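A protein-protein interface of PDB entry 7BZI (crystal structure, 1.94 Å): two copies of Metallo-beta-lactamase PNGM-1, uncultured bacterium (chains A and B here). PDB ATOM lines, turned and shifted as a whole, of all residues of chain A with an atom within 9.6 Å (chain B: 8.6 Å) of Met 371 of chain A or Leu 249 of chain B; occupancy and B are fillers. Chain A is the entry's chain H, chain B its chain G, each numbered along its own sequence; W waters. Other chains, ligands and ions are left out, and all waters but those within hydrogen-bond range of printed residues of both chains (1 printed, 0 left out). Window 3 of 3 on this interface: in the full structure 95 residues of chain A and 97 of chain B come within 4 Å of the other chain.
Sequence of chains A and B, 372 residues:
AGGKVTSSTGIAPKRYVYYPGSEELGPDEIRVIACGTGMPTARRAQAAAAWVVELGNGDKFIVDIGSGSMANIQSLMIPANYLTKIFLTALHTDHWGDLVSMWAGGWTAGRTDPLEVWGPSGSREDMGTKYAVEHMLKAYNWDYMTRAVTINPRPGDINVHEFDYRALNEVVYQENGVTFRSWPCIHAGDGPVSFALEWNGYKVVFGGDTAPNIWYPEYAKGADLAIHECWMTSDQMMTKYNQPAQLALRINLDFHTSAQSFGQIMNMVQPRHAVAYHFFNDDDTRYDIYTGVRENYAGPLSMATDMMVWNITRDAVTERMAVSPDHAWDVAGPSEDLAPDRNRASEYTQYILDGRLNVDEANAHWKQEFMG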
ATOM      1  N   ASN A 363       6.055  11.149   9.653  1.00  0.00           N
ATOM      2  CA  ASN A 363       6.878   9.970  10.046  1.00  0.00           C
ATOM      3  C   ASN A 363       8.169   9.909   9.217  1.00  0.00           C
ATOM      4  O   ASN A 363       8.977   8.985   9.460  1.00  0.00           O
ATOM      5  CB  ASN A 363       6.078   8.664   9.942  1.00  0.00           C
ATOM      6  CG  ASN A 363       4.998   8.544  11.000  1.00  0.00           C
ATOM      7  OD1 ASN A 363       5.216   7.950  12.056  1.00  0.00           O
ATOM      8  ND2 ASN A 363       3.828   9.103  10.733  1.00  0.00           N
ATOM      9  N   ALA A 364       8.377  10.863   8.302  1.00  0.00           N
ATOM     10  CA  ALA A 364       9.453  10.835   7.280  1.00  0.00           C
ATOM     11  C   ALA A 364      10.836  10.924   7.941  1.00  0.00           C
ATOM     12  O   ALA A 364      11.739  10.158   7.528  1.00  0.00           O
ATOM     13  CB  ALA A 364       9.245  11.955   6.289  1.00  0.00           C
ATOM     14  N   HIS A 365      11.003  11.832   8.912  1.00  0.00           N
ATOM     15  CA  HIS A 365      12.305  12.121   9.580  1.00  0.00           C
ATOM     16  C   HIS A 365      12.848  10.835  10.222  1.00  0.00           C
ATOM     17  O   HIS A 365      13.959  10.402   9.842  1.00  0.00           O
ATOM     18  CB  HIS A 365      12.169  13.292  10.574  1.00  0.00           C
ATOM     19  CG  HIS A 365      13.458  13.701  11.212  1.00  0.00           C
ATOM     20  ND1 HIS A 365      13.513  14.622  12.244  1.00  0.00           N
ATOM     21  CD2 HIS A 365      14.736  13.305  10.991  1.00  0.00           C
ATOM     22  CE1 HIS A 365      14.767  14.786  12.617  1.00  0.00           C
ATOM     23  NE2 HIS A 365      15.536  13.988  11.864  1.00  0.00           N
ATOM     24  N   TRP A 366      12.078  10.235  11.137  1.00  0.00           N
ATOM     25  CA  TRP A 366      12.507   9.064  11.954  1.00  0.00           C
ATOM     26  C   TRP A 366      12.670   7.836  11.049  1.00  0.00           C
ATOM     27  O   TRP A 366      13.624   7.062  11.282  1.00  0.00           O
ATOM     28  CB  TRP A 366      11.545   8.817  13.132  1.00  0.00           C
ATOM     29  CG  TRP A 366      10.334   7.973  12.847  1.00  0.00           C
ATOM     30  CD1 TRP A 366       9.049   8.407  12.695  1.00  0.00           C
ATOM     31  CD2 TRP A 366      10.285   6.541  12.722  1.00  0.00           C
ATOM     32  NE1 TRP A 366       8.213   7.350  12.463  1.00  0.00           N
ATOM     33  CE2 TRP A 366       8.941   6.192  12.481  1.00  0.00           C
ATOM     34  CE3 TRP A 366      11.242   5.521  12.791  1.00  0.00           C
ATOM     35  CZ2 TRP A 366       8.534   4.873  12.304  1.00  0.00           C
ATOM     36  CZ3 TRP A 366      10.841   4.218  12.616  1.00  0.00           C
ATOM     37  CH2 TRP A 366       9.504   3.902  12.365  1.00  0.00           C
ATOM     38  N   LYS A 367      11.778   7.685  10.060  1.00  0.00           N
ATOM     39  CA  LYS A 367      11.800   6.614   9.021  1.00  0.00           C
ATOM     40  C   LYS A 367      13.170   6.604   8.328  1.00  0.00           C
ATOM     41  O   LYS A 367      13.660   5.498   8.047  1.00  0.00           O
ATOM     42  CB  LYS A 367      10.668   6.841   8.012  1.00  0.00           C
ATOM     43  CG  LYS A 367      10.131   5.618   7.278  1.00  0.00           C
ATOM     44  CD  LYS A 367       8.639   5.743   6.990  1.00  0.00           C
ATOM     45  CE  LYS A 367       8.167   5.036   5.736  1.00  0.00           C
ATOM     46  NZ  LYS A 367       8.537   3.600   5.732  1.00  0.00           N
ATOM     47  N   GLN A 368      13.761   7.780   8.065  1.00  0.00           N
ATOM     48  CA  GLN A 368      15.128   7.912   7.486  1.00  0.00           C
ATOM     49  C   GLN A 368      16.170   7.388   8.489  1.00  0.00           C
ATOM     50  O   GLN A 368      16.931   6.459   8.123  1.00  0.00           O
ATOM     51  CB  GLN A 368      15.446   9.359   7.088  1.00  0.00           C
ATOM     52  CG  GLN A 368      16.871   9.791   7.444  1.00  0.00           C
ATOM     53  CD  GLN A 368      17.518  10.741   6.466  1.00  0.00           C
ATOM     54  OE1 GLN A 368      18.736  10.732   6.288  1.00  0.00           O
ATOM     55  NE2 GLN A 368      16.707  11.569   5.825  1.00  0.00           N
ATOM     56  N   GLU A 369      16.231   7.987   9.685  1.00  0.00           N
ATOM     57  CA  GLU A 369      17.221   7.658  10.750  1.00  0.00           C
ATOM     58  C   GLU A 369      17.220   6.135  10.969  1.00  0.00           C
ATOM     59  O   GLU A 369      18.292   5.507  10.806  1.00  0.00           O
ATOM     60  CB  GLU A 369      16.898   8.429  12.037  1.00  0.00           C
ATOM     61  CG  GLU A 369      18.114   8.786  12.885  1.00  0.00           C
ATOM     62  CD  GLU A 369      18.768   7.675  13.705  1.00  0.00           C
ATOM     63  OE1 GLU A 369      18.143   6.610  13.919  1.00  0.00           O
ATOM     64  OE2 GLU A 369      19.915   7.886  14.141  1.00  0.00           O
ATOM     65  N   PHE A 370      16.046   5.569  11.272  1.00  0.00           N
ATOM     66  CA  PHE A 370      15.845   4.150  11.670  1.00  0.00           C
ATOM     67  C   PHE A 370      16.404   3.196  10.606  1.00  0.00           C
ATOM     68  O   PHE A 370      17.125   2.242  10.967  1.00  0.00           O
ATOM     69  CB  PHE A 370      14.364   3.851  11.920  1.00  0.00           C
ATOM     70  CG  PHE A 370      14.100   2.489  12.515  1.00  0.00           C
ATOM     71  CD1 PHE A 370      14.345   2.240  13.859  1.00  0.00           C
ATOM     72  CD2 PHE A 370      13.615   1.453  11.730  1.00  0.00           C
ATOM     73  CE1 PHE A 370      14.116   0.984  14.398  1.00  0.00           C
ATOM     74  CE2 PHE A 370      13.379   0.201  12.274  1.00  0.00           C
ATOM     75  CZ  PHE A 370      13.629  -0.030  13.607  1.00  0.00           C
ATOM     76  N   MET A 371      16.078   3.432   9.333  1.00  0.00           N
ATOM     77  CA  MET A 371      16.429   2.511   8.217  1.00  0.00           C
ATOM     78  C   MET A 371      17.948   2.514   7.977  1.00  0.00           C
ATOM     79  O   MET A 371      18.455   1.483   7.479  1.00  0.00           O
ATOM     80  CB  MET A 371      15.661   2.888   6.947  1.00  0.00           C
ATOM     81  CG  MET A 371      14.173   2.643   7.096  1.00  0.00           C
ATOM     82  SD  MET A 371      13.175   3.132   5.671  1.00  0.00           S
ATOM     83  CE  MET A 371      12.977   1.548   4.852  1.00  0.00           C
ATOM     84  N   GLY A 372      18.645   3.599   8.350  1.00  0.00           N
ATOM     85  CA  GLY A 372      20.121   3.678   8.388  1.00  0.00           C
ATOM     86  C   GLY A 372      20.657   3.528   9.804  1.00  0.00           C
ATOM     87  O   GLY A 372      20.612   2.460  10.423  1.00  0.00           O
ATOM     88  N   MET B 232       4.900   2.746  21.480  1.00  0.00           N
ATOM     89  CA  MET B 232       6.359   2.721  21.746  1.00  0.00           C
ATOM     90  C   MET B 232       7.085   2.785  20.397  1.00  0.00           C
ATOM     91  O   MET B 232       6.463   2.505  19.352  1.00  0.00           O
ATOM     92  CB  MET B 232       6.768   1.477  22.545  1.00  0.00           C
ATOM     93  CG  MET B 232       6.082   1.427  23.917  1.00  0.00           C
ATOM     94  SD  MET B 232       6.611   0.063  24.966  1.00  0.00           S
ATOM     95  CE  MET B 232       6.273  -1.334  23.898  1.00  0.00           C
ATOM     96  N   THR B 233       8.343   3.195  20.424  1.00  0.00           N
ATOM     97  CA  THR B 233       9.140   3.502  19.217  1.00  0.00           C
ATOM     98  C   THR B 233       9.646   2.191  18.619  1.00  0.00           C
ATOM     99  O   THR B 233       9.740   1.199  19.365  1.00  0.00           O
ATOM    100  CB  THR B 233      10.302   4.453  19.535  1.00  0.00           C
ATOM    101  OG1 THR B 233      11.334   3.698  20.168  1.00  0.00           O
ATOM    102  CG2 THR B 233       9.876   5.630  20.385  1.00  0.00           C
ATOM    103  N   SER B 234      10.005   2.222  17.334  1.00  0.00           N
ATOM    104  CA  SER B 234      10.545   1.067  16.577  1.00  0.00           C
ATOM    105  C   SER B 234      11.907   0.665  17.162  1.00  0.00           C
ATOM    106  O   SER B 234      12.215  -0.555  17.157  1.00  0.00           O
ATOM    107  CB  SER B 234      10.584   1.384  15.096  1.00  0.00           C
ATOM    108  OG  SER B 234       9.262   1.630  14.620  1.00  0.00           O
ATOM    109  N   ASP B 235      12.684   1.626  17.689  1.00  0.00           N
ATOM    110  CA  ASP B 235      13.950   1.312  18.415  1.00  0.00           C
ATOM    111  C   ASP B 235      13.597   0.516  19.678  1.00  0.00           C
ATOM    112  O   ASP B 235      14.308  -0.465  19.974  1.00  0.00           O
ATOM    113  CB  ASP B 235      14.787   2.560  18.717  1.00  0.00           C
ATOM    114  CG  ASP B 235      15.614   3.034  17.529  1.00  0.00           C
ATOM    115  OD1 ASP B 235      16.254   2.173  16.871  1.00  0.00           O
ATOM    116  OD2 ASP B 235      15.600   4.261  17.253  1.00  0.00           O
ATOM    117  N   MET B 237      10.778  -1.348  20.170  1.00  0.00           N
ATOM    118  CA  MET B 237      10.326  -2.692  19.723  1.00  0.00           C
ATOM    119  C   MET B 237      11.549  -3.585  19.482  1.00  0.00           C
ATOM    120  O   MET B 237      11.424  -4.805  19.685  1.00  0.00           O
ATOM    121  CB  MET B 237       9.476  -2.632  18.446  1.00  0.00           C
ATOM    122  CG  MET B 237       8.151  -1.894  18.605  1.00  0.00           C
ATOM    123  SD  MET B 237       7.268  -2.255  20.155  1.00  0.00           S
ATOM    124  CE  MET B 237       6.023  -3.423  19.606  1.00  0.00           C
ATOM    125  N   MET B 238      12.696  -3.019  19.090  1.00  0.00           N
ATOM    126  CA  MET B 238      13.914  -3.815  18.769  1.00  0.00           C
ATOM    127  C   MET B 238      14.656  -4.211  20.058  1.00  0.00           C
ATOM    128  O   MET B 238      14.938  -5.408  20.219  1.00  0.00           O
ATOM    129  CB  MET B 238      14.849  -3.053  17.825  1.00  0.00           C
ATOM    130  CG  MET B 238      14.422  -3.131  16.365  1.00  0.00           C
ATOM    131  SD  MET B 238      15.725  -2.558  15.231  1.00  0.00           S
ATOM    132  CE  MET B 238      16.873  -3.938  15.250  1.00  0.00           C
ATOM    133  N   GLN B 243      12.935  -7.716  18.007  1.00  0.00           N
ATOM    134  CA  GLN B 243      12.256  -7.764  16.683  1.00  0.00           C
ATOM    135  C   GLN B 243      13.254  -7.394  15.588  1.00  0.00           C
ATOM    136  O   GLN B 243      14.207  -6.652  15.842  1.00  0.00           O
ATOM    137  CB  GLN B 243      11.062  -6.807  16.652  1.00  0.00           C
ATOM    138  CG  GLN B 243      10.019  -7.076  17.728  1.00  0.00           C
ATOM    139  CD  GLN B 243       8.710  -7.569  17.166  1.00  0.00           C
ATOM    140  OE1 GLN B 243       7.672  -6.932  17.325  1.00  0.00           O
ATOM    141  NE2 GLN B 243       8.755  -8.708  16.494  1.00  0.00           N
ATOM    142  N   PRO B 244      13.065  -7.898  14.344  1.00  0.00           N
ATOM    143  CA  PRO B 244      13.899  -7.491  13.214  1.00  0.00           C
ATOM    144  C   PRO B 244      13.523  -6.066  12.779  1.00  0.00           C
ATOM    145  O   PRO B 244      12.375  -5.684  12.979  1.00  0.00           O
ATOM    146  CB  PRO B 244      13.573  -8.529  12.129  1.00  0.00           C
ATOM    147  CG  PRO B 244      12.148  -8.948  12.438  1.00  0.00           C
ATOM    148  CD  PRO B 244      12.021  -8.860  13.948  1.00  0.00           C
ATOM    149  N   ALA B 245      14.484  -5.333  12.200  1.00  0.00           N
ATOM    150  CA  ALA B 245      14.364  -3.912  11.785  1.00  0.00           C
ATOM    151  C   ALA B 245      13.050  -3.671  11.025  1.00  0.00           C
ATOM    152  O   ALA B 245      12.349  -2.709  11.380  1.00  0.00           O
ATOM    153  CB  ALA B 245      15.561  -3.512  10.957  1.00  0.00           C
ATOM    154  N   GLN B 246      12.725  -4.499  10.022  1.00  0.00           N
ATOM    155  CA  GLN B 246      11.605  -4.233   9.074  1.00  0.00           C
ATOM    156  C   GLN B 246      10.272  -4.413   9.815  1.00  0.00           C
ATOM    157  O   GLN B 246       9.402  -3.529   9.649  1.00  0.00           O
ATOM    158  CB  GLN B 246      11.759  -5.048   7.777  1.00  0.00           C
ATOM    159  CG  GLN B 246      11.036  -6.396   7.739  1.00  0.00           C
ATOM    160  CD  GLN B 246       9.730  -6.385   6.972  1.00  0.00           C
ATOM    161  OE1 GLN B 246       9.516  -5.567   6.079  1.00  0.00           O
ATOM    162  NE2 GLN B 246       8.847  -7.319   7.299  1.00  0.00           N
ATOM    163  N   LEU B 247      10.119  -5.462  10.636  1.00  0.00           N
ATOM    164  CA  LEU B 247       8.883  -5.678  11.448  1.00  0.00           C
ATOM    165  C   LEU B 247       8.732  -4.534  12.462  1.00  0.00           C
ATOM    166  O   LEU B 247       7.589  -4.070  12.657  1.00  0.00           O
ATOM    167  CB  LEU B 247       8.919  -7.037  12.158  1.00  0.00           C
ATOM    168  CG  LEU B 247       8.012  -8.116  11.561  1.00  0.00           C
ATOM    169  CD1 LEU B 247       8.667  -8.774  10.350  1.00  0.00           C
ATOM    170  CD2 LEU B 247       7.641  -9.157  12.614  1.00  0.00           C
ATOM    171  N   ALA B 248       9.844  -4.096  13.065  1.00  0.00           N
ATOM    172  CA  ALA B 248       9.912  -2.956  14.012  1.00  0.00           C
ATOM    173  C   ALA B 248       9.364  -1.691  13.330  1.00  0.00           C
ATOM    174  O   ALA B 248       8.491  -1.012  13.940  1.00  0.00           O
ATOM    175  CB  ALA B 248      11.331  -2.773  14.496  1.00  0.00           C
ATOM    176  N   LEU B 249       9.839  -1.407  12.106  1.00  0.00           N
ATOM    177  CA  LEU B 249       9.403  -0.258  11.259  1.00  0.00           C
ATOM    178  C   LEU B 249       7.900  -0.375  10.968  1.00  0.00           C
ATOM    179  O   LEU B 249       7.180   0.629  11.174  1.00  0.00           O
ATOM    180  CB  LEU B 249      10.217  -0.235   9.959  1.00  0.00           C
ATOM    181  CG  LEU B 249       9.968   0.960   9.032  1.00  0.00           C
ATOM    182  CD1 LEU B 249      10.747   2.185   9.495  1.00  0.00           C
ATOM    183  CD2 LEU B 249      10.330   0.619   7.592  1.00  0.00           C
ATOM    184  N   ARG B 250       7.451  -1.557  10.532  1.00  0.00           N
ATOM    185  CA  ARG B 250       6.057  -1.815  10.066  1.00  0.00           C
ATOM    186  C   ARG B 250       5.074  -1.569  11.224  1.00  0.00           C
ATOM    187  O   ARG B 250       3.982  -1.034  10.961  1.00  0.00           O
ATOM    188  CB  ARG B 250       5.921  -3.233   9.487  1.00  0.00           C
ATOM    189  CG  ARG B 250       6.587  -3.459   8.130  1.00  0.00           C
ATOM    190  CD  ARG B 250       5.899  -2.755   6.967  1.00  0.00           C
ATOM    191  NE  ARG B 250       6.454  -1.425   6.705  1.00  0.00           N
ATOM    192  CZ  ARG B 250       5.851  -0.434   6.036  1.00  0.00           C
ATOM    193  NH1 ARG B 250       4.633  -0.585   5.538  1.00  0.00           N
ATOM    194  NH2 ARG B 250       6.478   0.720   5.873  1.00  0.00           N
ATOM    195  N   ILE B 251       5.451  -1.915  12.461  1.00  0.00           N
ATOM    196  CA  ILE B 251       4.572  -1.798  13.666  1.00  0.00           C
ATOM    197  C   ILE B 251       4.085  -0.345  13.830  1.00  0.00           C
ATOM    198  O   ILE B 251       2.883  -0.163  14.194  1.00  0.00           O
ATOM    199  CB  ILE B 251       5.288  -2.350  14.922  1.00  0.00           C
ATOM    200  CG1 ILE B 251       5.208  -3.881  14.981  1.00  0.00           C
ATOM    201  CG2 ILE B 251       4.734  -1.710  16.191  1.00  0.00           C
ATOM    202  CD1 ILE B 251       6.151  -4.525  15.984  1.00  0.00           C
ATOM    203  N   ASN B 252       4.960   0.642  13.564  1.00  0.00           N
ATOM    204  CA  ASN B 252       4.723   2.097  13.804  1.00  0.00           C
ATOM    205  C   ASN B 252       4.115   2.760  12.557  1.00  0.00           C
ATOM    206  O   ASN B 252       3.568   3.879  12.707  1.00  0.00           O
ATOM    207  CB  ASN B 252       6.003   2.802  14.273  1.00  0.00           C
ATOM    208  CG  ASN B 252       6.117   2.825  15.783  1.00  0.00           C
ATOM    209  OD1 ASN B 252       5.333   3.501  16.452  1.00  0.00           O
ATOM    210  ND2 ASN B 252       7.069   2.078  16.327  1.00  0.00           N
ATOM    211  N   LEU B 253       4.175   2.095  11.392  1.00  0.00           N
ATOM    212  CA  LEU B 253       3.545   2.553  10.115  1.00  0.00           C
ATOM    213  C   LEU B 253       2.217   1.810   9.865  1.00  0.00           C
ATOM    214  O   LEU B 253       1.186   2.491   9.685  1.00  0.00           O
ATOM    215  CB  LEU B 253       4.528   2.339   8.958  1.00  0.00           C
ATOM    216  CG  LEU B 253       5.540   3.461   8.701  1.00  0.00           C
ATOM    217  CD1 LEU B 253       4.854   4.808   8.512  1.00  0.00           C
ATOM    218  CD2 LEU B 253       6.581   3.549   9.804  1.00  0.00           C
ATOM    219  N   ASP B 254       2.226   0.470   9.879  1.00  0.00           N
ATOM    220  CA  ASP B 254       1.099  -0.388   9.403  1.00  0.00           C
ATOM    221  C   ASP B 254       0.019  -0.533  10.483  1.00  0.00           C
ATOM    222  O   ASP B 254      -1.154  -0.312  10.154  1.00  0.00           O
ATOM    223  CB  ASP B 254       1.573  -1.780   8.962  1.00  0.00           C
ATOM    224  CG  ASP B 254       2.339  -1.823   7.645  1.00  0.00           C
ATOM    225  OD1 ASP B 254       2.578  -0.740   7.054  1.00  0.00           O
ATOM    226  OD2 ASP B 254       2.693  -2.952   7.207  1.00  0.00           O
ATOM    227  N   PHE B 255       0.406  -0.902  11.710  1.00  0.00           N
ATOM    228  CA  PHE B 255      -0.473  -1.517  12.743  1.00  0.00           C
ATOM    229  C   PHE B 255      -0.965  -0.484  13.774  1.00  0.00           C
ATOM    230  O   PHE B 255      -2.162  -0.508  14.156  1.00  0.00           O
ATOM    231  CB  PHE B 255       0.297  -2.671  13.390  1.00  0.00           C
ATOM    232  CG  PHE B 255       0.791  -3.729  12.426  1.00  0.00           C
ATOM    233  CD1 PHE B 255      -0.099  -4.445  11.633  1.00  0.00           C
ATOM    234  CD2 PHE B 255       2.143  -4.038  12.330  1.00  0.00           C
ATOM    235  CE1 PHE B 255       0.356  -5.423  10.759  1.00  0.00           C
ATOM    236  CE2 PHE B 255       2.596  -5.022  11.460  1.00  0.00           C
ATOM    237  CZ  PHE B 255       1.700  -5.708  10.671  1.00  0.00           C
ATOM    238  N   HIS B 256      -0.084   0.415  14.226  1.00  0.00           N
ATOM    239  CA  HIS B 256      -0.359   1.356  15.346  1.00  0.00           C
ATOM    240  C   HIS B 256      -0.096   2.805  14.944  1.00  0.00           C
ATOM    241  O   HIS B 256       0.530   3.035  13.896  1.00  0.00           O
ATOM    242  CB  HIS B 256       0.483   0.968  16.563  1.00  0.00           C
ATOM    243  CG  HIS B 256       0.111  -0.374  17.084  1.00  0.00           C
ATOM    244  ND1 HIS B 256      -1.113  -0.603  17.701  1.00  0.00           N
ATOM    245  CD2 HIS B 256       0.751  -1.562  17.007  1.00  0.00           C
ATOM    246  CE1 HIS B 256      -1.194  -1.877  18.019  1.00  0.00           C
ATOM    247  NE2 HIS B 256      -0.063  -2.490  17.601  1.00  0.00           N
ATOM    248  N   SER B 258       2.110   5.701  15.601  1.00  0.00           N
ATOM    249  CA  SER B 258       3.435   6.202  16.064  1.00  0.00           C
ATOM    250  C   SER B 258       3.231   7.464  16.908  1.00  0.00           C
ATOM    251  O   SER B 258       2.170   8.132  16.745  1.00  0.00           O
ATOM    252  CB  SER B 258       4.337   6.506  14.887  1.00  0.00           C
ATOM    253  OG  SER B 258       3.887   7.690  14.247  1.00  0.00           O
HETATM  254  O   HOH W   1      17.761   4.170  15.564  1.00  0.00           O
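No position is printed for both chains.
The side-chain hydroxyl (OG) of Ser 234 of chain B sits at hydrogen-bond distance from the backbone carbonyl oxygen (O) of Ala 248 of chain B (2.8 Å).
The side-chain amide nitrogen (ND2) of Asn 252 of chain B lies within hydrogen-bond range of the backbone carbonyl oxygen (O) of Met 232 of chain B (3.1 Å).
The side-chain hydroxyl (OG) of Ser 234 of chain B is in hydrogen-bond range of the side-chain amide nitrogen (ND2) of Asn 252 of chain B (2.8 Å).
OD1 of Asp 254 of chain B is in salt-bridge range of NH1 of Arg 250 of chain B, 2.6 Å away.
The side-chain amide oxygen (OD1) of Asn 363 of chain A sits at hydrogen-bond distance from the indole nitrogen (NE1) of Trp 366 of chain A, 3.1 Å away.
Of chain B, only Leu 249 (3.9 Å) comes within 4 Å of Met 371 of chain A.
Gly 372 of chain A touches none of the printed residues of chain B.
Printed residues of chain B within 4 Å of Asn 363 of chain A: Ser 258.
Of the printed residues of chain A, Asn 252 of chain B touches Trp 366.
Leu 247 of chain B touches none of the printed residues of chain A.
The nearest printed residue of chain A that does not touch Asp 235 of chain B is Glu 369 of chain A (4.8 Å).
The side-chain hydroxyl (OG) of Ser 258 of chain B lies within hydrogen-bond range of the side-chain amide oxygen (OD1) of Asn 363 of chain A (2.6 Å).
Printed residues of chain B that touch a printed residue of chain A: Ser 234, Asp 235, Met 238, Ala 245, Ala 248, Leu 249, Arg 250, Asn 252, Leu 253 and Ser 258.
Hydrophobic or aromatic side chains of chain B within 4 Å of the printed part of chain A: Met 238, Ala 248, Leu 249 and Leu 253.
Of the 10 printed residues of chain A, 5 touch a printed residue of chain B.
Printed residues of chain A that touch a printed residue of chain B: Asn 363, Trp 366, Lys 367, Phe 370 and Met 371.
Hydrophobic or aromatic side chains of chain A that line the printed part of chain B: Trp 366, Phe 370 and Met 371.
Along chain A the printed residues that touch a printed residue of chain B span positions 363 to 371.
Trp 366 of chain A touches Ser 234 of chain B (CH2 to OG, 3.2 Å).
Trp 366 of chain A touches Asn 252 of chain B (CZ2 to CB, 3.8 Å).
Trp 366 of chain A touches Leu 253 of chain B (CZ2 to CD2, 3.4 Å).
NZ of Lys 367 of chain A touches CD2 of Leu 249 of chain B, at 3.9 Å.
NH2 of Arg 250 of chain B touches NZ of Lys 367 of chain A, 3.5 Å away.
Ser 234 of chain B touches Phe 370 of chain A.
CZ of Phe 370 of chain A touches SD of Met 238 of chain B, 3.7 Å away.
CE2 of Phe 370 of chain A touches O of Ala 245 of chain B, at 3.2 Å.
Phe 370 of chain A touches Leu 249 of chain B.
CE of Met 371 of chain A touches CD2 of Leu 249 of chain B, at 3.9 Å.
Water W1 bridges the side-chain carboxylate of Asp 235 of chain B (2.7 Å) and the side-chain carboxylate of Glu 369 of chain A (3.0 Å).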
